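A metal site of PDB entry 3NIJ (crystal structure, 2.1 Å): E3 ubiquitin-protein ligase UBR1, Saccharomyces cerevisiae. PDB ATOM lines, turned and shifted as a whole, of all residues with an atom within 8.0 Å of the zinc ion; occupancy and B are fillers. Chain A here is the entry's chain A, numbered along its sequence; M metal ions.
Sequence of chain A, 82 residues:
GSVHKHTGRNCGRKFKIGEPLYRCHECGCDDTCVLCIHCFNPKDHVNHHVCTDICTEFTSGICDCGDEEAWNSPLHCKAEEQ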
ATOM      1  N   ARG A  23      13.754   9.879 -29.465  1.00  0.00           N
ATOM      2  CA  ARG A  23      13.668   9.068 -28.244  1.00  0.00           C
ATOM      3  C   ARG A  23      14.527   9.678 -27.146  1.00  0.00           C
ATOM      4  O   ARG A  23      15.521  10.345 -27.426  1.00  0.00           O
ATOM      5  CB  ARG A  23      14.152   7.638 -28.507  1.00  0.00           C
ATOM      6  CG  ARG A  23      13.238   6.804 -29.373  1.00  0.00           C
ATOM      7  CD  ARG A  23      13.641   5.344 -29.323  1.00  0.00           C
ATOM      8  NE  ARG A  23      14.879   5.088 -30.065  1.00  0.00           N
ATOM      9  CZ  ARG A  23      14.969   4.372 -31.180  1.00  0.00           C
ATOM     10  NH1 ARG A  23      13.876   3.811 -31.709  1.00  0.00           N
ATOM     11  NH2 ARG A  23      16.141   4.198 -31.775  1.00  0.00           N
ATOM     12  N   CYS A  24      14.148   9.449 -25.900  1.00  0.00           N
ATOM     13  CA  CYS A  24      14.925   9.930 -24.773  1.00  0.00           C
ATOM     14  C   CYS A  24      15.124   8.818 -23.758  1.00  0.00           C
ATOM     15  O   CYS A  24      14.158   8.264 -23.235  1.00  0.00           O
ATOM     16  CB  CYS A  24      14.252  11.142 -24.123  1.00  0.00           C
ATOM     17  SG  CYS A  24      15.212  11.869 -22.785  1.00  0.00           S
ATOM     18  N   HIS A  25      16.390   8.492 -23.470  1.00  0.00           N
ATOM     19  CA  HIS A  25      16.724   7.405 -22.559  1.00  0.00           C
ATOM     20  C   HIS A  25      16.040   7.569 -21.201  1.00  0.00           C
ATOM     21  O   HIS A  25      15.448   6.616 -20.690  1.00  0.00           O
ATOM     22  CB  HIS A  25      18.241   7.269 -22.389  1.00  0.00           C
ATOM     23  CG  HIS A  25      18.640   6.169 -21.452  1.00  0.00           C
ATOM     24  ND1 HIS A  25      18.567   4.829 -21.793  1.00  0.00           N
ATOM     25  CD2 HIS A  25      19.119   6.206 -20.184  1.00  0.00           C
ATOM     26  CE1 HIS A  25      18.975   4.091 -20.769  1.00  0.00           C
ATOM     27  NE2 HIS A  25      19.311   4.906 -19.784  1.00  0.00           N
ATOM     28  N   GLU A  26      16.134   8.772 -20.642  1.00  0.00           N
ATOM     29  CA  GLU A  26      15.550   9.098 -19.333  1.00  0.00           C
ATOM     30  C   GLU A  26      14.019   9.197 -19.351  1.00  0.00           C
ATOM     31  O   GLU A  26      13.357   8.595 -18.498  1.00  0.00           O
ATOM     32  CB  GLU A  26      16.147  10.414 -18.809  1.00  0.00           C
ATOM     33  CG  GLU A  26      17.638  10.341 -18.425  1.00  0.00           C
ATOM     34  CD  GLU A  26      18.552  10.141 -19.625  1.00  0.00           C
ATOM     35  OE1 GLU A  26      18.316  10.764 -20.688  1.00  0.00           O
ATOM     36  OE2 GLU A  26      19.525   9.358 -19.500  1.00  0.00           O
ATOM     37  N   CYS A  27      13.464   9.941 -20.321  1.00  0.00           N
ATOM     38  CA  CYS A  27      12.036  10.242 -20.334  1.00  0.00           C
ATOM     39  C   CYS A  27      11.181   9.076 -20.842  1.00  0.00           C
ATOM     40  O   CYS A  27      10.065   8.881 -20.388  1.00  0.00           O
ATOM     41  CB  CYS A  27      11.746  11.511 -21.149  1.00  0.00           C
ATOM     42  SG  CYS A  27      12.707  12.951 -20.637  1.00  0.00           S
ATOM     43  N   GLY A  28      11.730   8.315 -21.792  1.00  0.00           N
ATOM     44  CA  GLY A  28      11.029   7.163 -22.357  1.00  0.00           C
ATOM     45  C   GLY A  28      10.925   5.978 -21.417  1.00  0.00           C
ATOM     46  O   GLY A  28      11.913   5.570 -20.802  1.00  0.00           O
ATOM     47  N   LEU A  35       8.766  10.479 -30.060  1.00  0.00           N
ATOM     48  CA  LEU A  35       8.152  11.789 -30.314  1.00  0.00           C
ATOM     49  C   LEU A  35       8.429  12.230 -31.747  1.00  0.00           C
ATOM     50  O   LEU A  35       9.514  12.002 -32.273  1.00  0.00           O
ATOM     51  CB  LEU A  35       8.714  12.841 -29.362  1.00  0.00           C
ATOM     52  CG  LEU A  35       8.408  12.698 -27.862  1.00  0.00           C
ATOM     53  CD1 LEU A  35       9.387  13.498 -27.020  1.00  0.00           C
ATOM     54  CD2 LEU A  35       6.981  13.113 -27.567  1.00  0.00           C
ATOM     55  N   PHE A  40       8.351  17.027 -30.164  1.00  0.00           N
ATOM     56  CA  PHE A  40       9.597  17.084 -29.406  1.00  0.00           C
ATOM     57  C   PHE A  40      10.011  18.515 -29.049  1.00  0.00           C
ATOM     58  O   PHE A  40      10.192  19.372 -29.925  1.00  0.00           O
ATOM     59  CB  PHE A  40      10.732  16.369 -30.149  1.00  0.00           C
ATOM     60  CG  PHE A  40      12.073  16.405 -29.442  1.00  0.00           C
ATOM     61  CD1 PHE A  40      12.375  15.490 -28.447  1.00  0.00           C
ATOM     62  CD2 PHE A  40      13.027  17.365 -29.781  1.00  0.00           C
ATOM     63  CE1 PHE A  40      13.620  15.518 -27.799  1.00  0.00           C
ATOM     64  CE2 PHE A  40      14.265  17.415 -29.135  1.00  0.00           C
ATOM     65  CZ  PHE A  40      14.551  16.481 -28.139  1.00  0.00           C
ATOM     66  N   ASN A  41      10.131  18.761 -27.748  1.00  0.00           N
ATOM     67  CA  ASN A  41      10.541  20.059 -27.233  1.00  0.00           C
ATOM     68  C   ASN A  41      11.901  19.935 -26.559  1.00  0.00           C
ATOM     69  O   ASN A  41      12.026  19.235 -25.561  1.00  0.00           O
ATOM     70  CB  ASN A  41       9.488  20.595 -26.251  1.00  0.00           C
ATOM     71  CG  ASN A  41       9.549  22.114 -26.084  1.00  0.00           C
ATOM     72  OD1 ASN A  41      10.612  22.721 -26.201  1.00  0.00           O
ATOM     73  ND2 ASN A  41       8.405  22.717 -25.818  1.00  0.00           N
ATOM     74  N   PRO A  42      12.929  20.603 -27.124  1.00  0.00           N
ATOM     75  CA  PRO A  42      14.282  20.560 -26.549  1.00  0.00           C
ATOM     76  C   PRO A  42      14.309  21.034 -25.099  1.00  0.00           C
ATOM     77  O   PRO A  42      15.142  20.580 -24.314  1.00  0.00           O
ATOM     78  CB  PRO A  42      15.070  21.542 -27.431  1.00  0.00           C
ATOM     79  CG  PRO A  42      14.312  21.620 -28.700  1.00  0.00           C
ATOM     80  CD  PRO A  42      12.865  21.441 -28.338  1.00  0.00           C
ATOM     81  N   LYS A  43      13.377  21.918 -24.764  1.00  0.00           N
ATOM     82  CA  LYS A  43      13.207  22.464 -23.413  1.00  0.00           C
ATOM     83  C   LYS A  43      12.994  21.354 -22.376  1.00  0.00           C
ATOM     84  O   LYS A  43      13.346  21.517 -21.205  1.00  0.00           O
ATOM     85  CB  LYS A  43      12.008  23.412 -23.407  1.00  0.00           C
ATOM     86  CG  LYS A  43      11.932  24.395 -22.250  1.00  0.00           C
ATOM     87  CD  LYS A  43      10.612  25.168 -22.327  1.00  0.00           C
ATOM     88  CE  LYS A  43      10.445  26.143 -21.180  1.00  0.00           C
ATOM     89  NZ  LYS A  43       9.088  26.764 -21.192  1.00  0.00           N
ATOM     90  N   ASP A  44      12.403  20.236 -22.813  1.00  0.00           N
ATOM     91  CA  ASP A  44      12.116  19.106 -21.941  1.00  0.00           C
ATOM     92  C   ASP A  44      13.338  18.222 -21.655  1.00  0.00           C
ATOM     93  O   ASP A  44      13.322  17.460 -20.680  1.00  0.00           O
ATOM     94  CB  ASP A  44      11.015  18.226 -22.562  1.00  0.00           C
ATOM     95  CG  ASP A  44       9.646  18.905 -22.550  1.00  0.00           C
ATOM     96  OD1 ASP A  44       9.372  19.689 -21.620  1.00  0.00           O
ATOM     97  OD2 ASP A  44       8.836  18.622 -23.462  1.00  0.00           O
ATOM     98  N   HIS A  45      14.372  18.323 -22.475  1.00  0.00           N
ATOM     99  CA  HIS A  45      15.448  17.321 -22.492  1.00  0.00           C
ATOM    100  C   HIS A  45      16.885  17.886 -22.460  1.00  0.00           C
ATOM    101  O   HIS A  45      17.794  17.304 -23.065  1.00  0.00           O
ATOM    102  CB  HIS A  45      15.280  16.385 -23.696  1.00  0.00           C
ATOM    103  CG  HIS A  45      13.879  15.896 -23.885  1.00  0.00           C
ATOM    104  ND1 HIS A  45      13.324  14.882 -23.136  1.00  0.00           N
ATOM    105  CD2 HIS A  45      12.908  16.297 -24.737  1.00  0.00           C
ATOM    106  CE1 HIS A  45      12.078  14.671 -23.526  1.00  0.00           C
ATOM    107  NE2 HIS A  45      11.794  15.528 -24.495  1.00  0.00           N
ATOM    108  N   VAL A  46      17.076  18.973 -21.728  1.00  0.00           N
ATOM    109  CA  VAL A  46      18.417  19.577 -21.572  1.00  0.00           C
ATOM    110  C   VAL A  46      19.368  18.572 -20.925  1.00  0.00           C
ATOM    111  O   VAL A  46      19.097  18.054 -19.838  1.00  0.00           O
ATOM    112  CB  VAL A  46      18.366  20.891 -20.759  1.00  0.00           C
ATOM    113  CG1 VAL A  46      19.754  21.547 -20.686  1.00  0.00           C
ATOM    114  CG2 VAL A  46      17.355  21.866 -21.376  1.00  0.00           C
ATOM    115  N   ASN A  47      20.479  18.301 -21.616  1.00  0.00           N
ATOM    116  CA  ASN A  47      21.492  17.332 -21.185  1.00  0.00           C
ATOM    117  C   ASN A  47      20.982  15.893 -20.967  1.00  0.00           C
ATOM    118  O   ASN A  47      21.669  15.055 -20.387  1.00  0.00           O
ATOM    119  CB  ASN A  47      22.283  17.844 -19.964  1.00  0.00           C
ATOM    120  CG  ASN A  47      23.178  19.057 -20.306  1.00  0.00           C
ATOM    121  OD1 ASN A  47      23.336  19.957 -19.488  1.00  0.00           O
ATOM    122  ND2 ASN A  47      23.733  19.077 -21.531  1.00  0.00           N
ATOM    123  N   HIS A  48      19.761  15.634 -21.441  1.00  0.00           N
ATOM    124  CA  HIS A  48      19.218  14.273 -21.504  1.00  0.00           C
ATOM    125  C   HIS A  48      19.891  13.515 -22.648  1.00  0.00           C
ATOM    126  O   HIS A  48      20.580  14.121 -23.485  1.00  0.00           O
ATOM    127  CB  HIS A  48      17.693  14.309 -21.679  1.00  0.00           C
ATOM    128  CG  HIS A  48      16.955  14.676 -20.434  1.00  0.00           C
ATOM    129  ND1 HIS A  48      15.598  14.442 -20.271  1.00  0.00           N
ATOM    130  CD2 HIS A  48      17.382  15.219 -19.263  1.00  0.00           C
ATOM    131  CE1 HIS A  48      15.226  14.857 -19.070  1.00  0.00           C
ATOM    132  NE2 HIS A  48      16.288  15.329 -18.441  1.00  0.00           N
ATOM    133  N   HIS A  49      19.721  12.196 -22.669  1.00  0.00           N
ATOM    134  CA  HIS A  49      20.346  11.392 -23.707  1.00  0.00           C
ATOM    135  C   HIS A  49      19.368  11.142 -24.845  1.00  0.00           C
ATOM    136  O   HIS A  49      18.698  10.104 -24.908  1.00  0.00           O
ATOM    137  CB  HIS A  49      20.913  10.105 -23.115  1.00  0.00           C
ATOM    138  CG  HIS A  49      22.101  10.329 -22.230  1.00  0.00           C
ATOM    139  ND1 HIS A  49      21.984  10.615 -20.891  1.00  0.00           N
ATOM    140  CD2 HIS A  49      23.427  10.333 -22.511  1.00  0.00           C
ATOM    141  CE1 HIS A  49      23.195  10.775 -20.377  1.00  0.00           C
ATOM    142  NE2 HIS A  49      24.081  10.612 -21.330  1.00  0.00           N
ATOM    143  N   VAL A  50      19.281  12.125 -25.737  1.00  0.00           N
ATOM    144  CA  VAL A  50      18.305  12.130 -26.818  1.00  0.00           C
ATOM    145  C   VAL A  50      18.876  11.487 -28.068  1.00  0.00           C
ATOM    146  O   VAL A  50      19.971  11.829 -28.529  1.00  0.00           O
ATOM    147  CB  VAL A  50      17.781  13.562 -27.120  1.00  0.00           C
ATOM    148  CG1 VAL A  50      16.779  13.546 -28.289  1.00  0.00           C
ATOM    149  CG2 VAL A  50      17.127  14.157 -25.890  1.00  0.00           C
ATOM    150  N   TRP A  71       5.819   7.748 -20.892  1.00  0.00           N
ATOM    151  CA  TRP A  71       6.799   8.726 -20.391  1.00  0.00           C
ATOM    152  C   TRP A  71       6.915   8.754 -18.862  1.00  0.00           C
ATOM    153  O   TRP A  71       5.933   8.556 -18.152  1.00  0.00           O
ATOM    154  CB  TRP A  71       6.484  10.122 -20.947  1.00  0.00           C
ATOM    155  CG  TRP A  71       6.326  10.092 -22.444  1.00  0.00           C
ATOM    156  CD1 TRP A  71       5.152  10.106 -23.137  1.00  0.00           C
ATOM    157  CD2 TRP A  71       7.362   9.957 -23.421  1.00  0.00           C
ATOM    158  NE1 TRP A  71       5.394  10.014 -24.495  1.00  0.00           N
ATOM    159  CE2 TRP A  71       6.748   9.918 -24.700  1.00  0.00           C
ATOM    160  CE3 TRP A  71       8.769   9.872 -23.347  1.00  0.00           C
ATOM    161  CZ2 TRP A  71       7.473   9.798 -25.887  1.00  0.00           C
ATOM    162  CZ3 TRP A  71       9.494   9.752 -24.534  1.00  0.00           C
ATOM    163  CH2 TRP A  71       8.852   9.720 -25.782  1.00  0.00           C
ATOM    164  N   SER A  73       8.428  11.485 -17.246  1.00  0.00           N
ATOM    165  CA  SER A  73       8.274  12.895 -16.869  1.00  0.00           C
ATOM    166  C   SER A  73       7.146  13.532 -17.681  1.00  0.00           C
ATOM    167  O   SER A  73       6.845  13.085 -18.787  1.00  0.00           O
ATOM    168  CB  SER A  73       9.576  13.660 -17.094  1.00  0.00           C
ATOM    169  OG  SER A  73      10.598  13.210 -16.228  1.00  0.00           O
ATOM    170  N   LEU A  75       5.628  15.868 -20.254  1.00  0.00           N
ATOM    171  CA  LEU A  75       6.173  16.545 -21.427  1.00  0.00           C
ATOM    172  C   LEU A  75       5.371  17.806 -21.741  1.00  0.00           C
ATOM    173  O   LEU A  75       4.235  17.961 -21.279  1.00  0.00           O
ATOM    174  CB  LEU A  75       6.200  15.610 -22.642  1.00  0.00           C
ATOM    175  CG  LEU A  75       7.126  14.385 -22.589  1.00  0.00           C
ATOM    176  CD1 LEU A  75       6.983  13.574 -23.868  1.00  0.00           C
ATOM    177  CD2 LEU A  75       8.595  14.746 -22.364  1.00  0.00           C
HETATM  178 ZN    ZN M   1      14.223  13.552 -21.892  1.00  0.00          ZN
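Four residues have an atom within 4 Å of the zinc ion: Cys 24, Cys 27, His 45 and His 48.
The nearest printed residue that does not touch the zinc ion is Asp 44 (4.2 Å).
A ring nitrogen (ND1) of His 45 is bound to the zinc ion.
The side-chain sulfur (SG) of Cys 27 binds the zinc ion (2.1 Å).
SG of Cys 24 binds the zinc ion (2.1 Å).
The zinc ion is bound by ND1 of His 48, at 2.3 Å.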
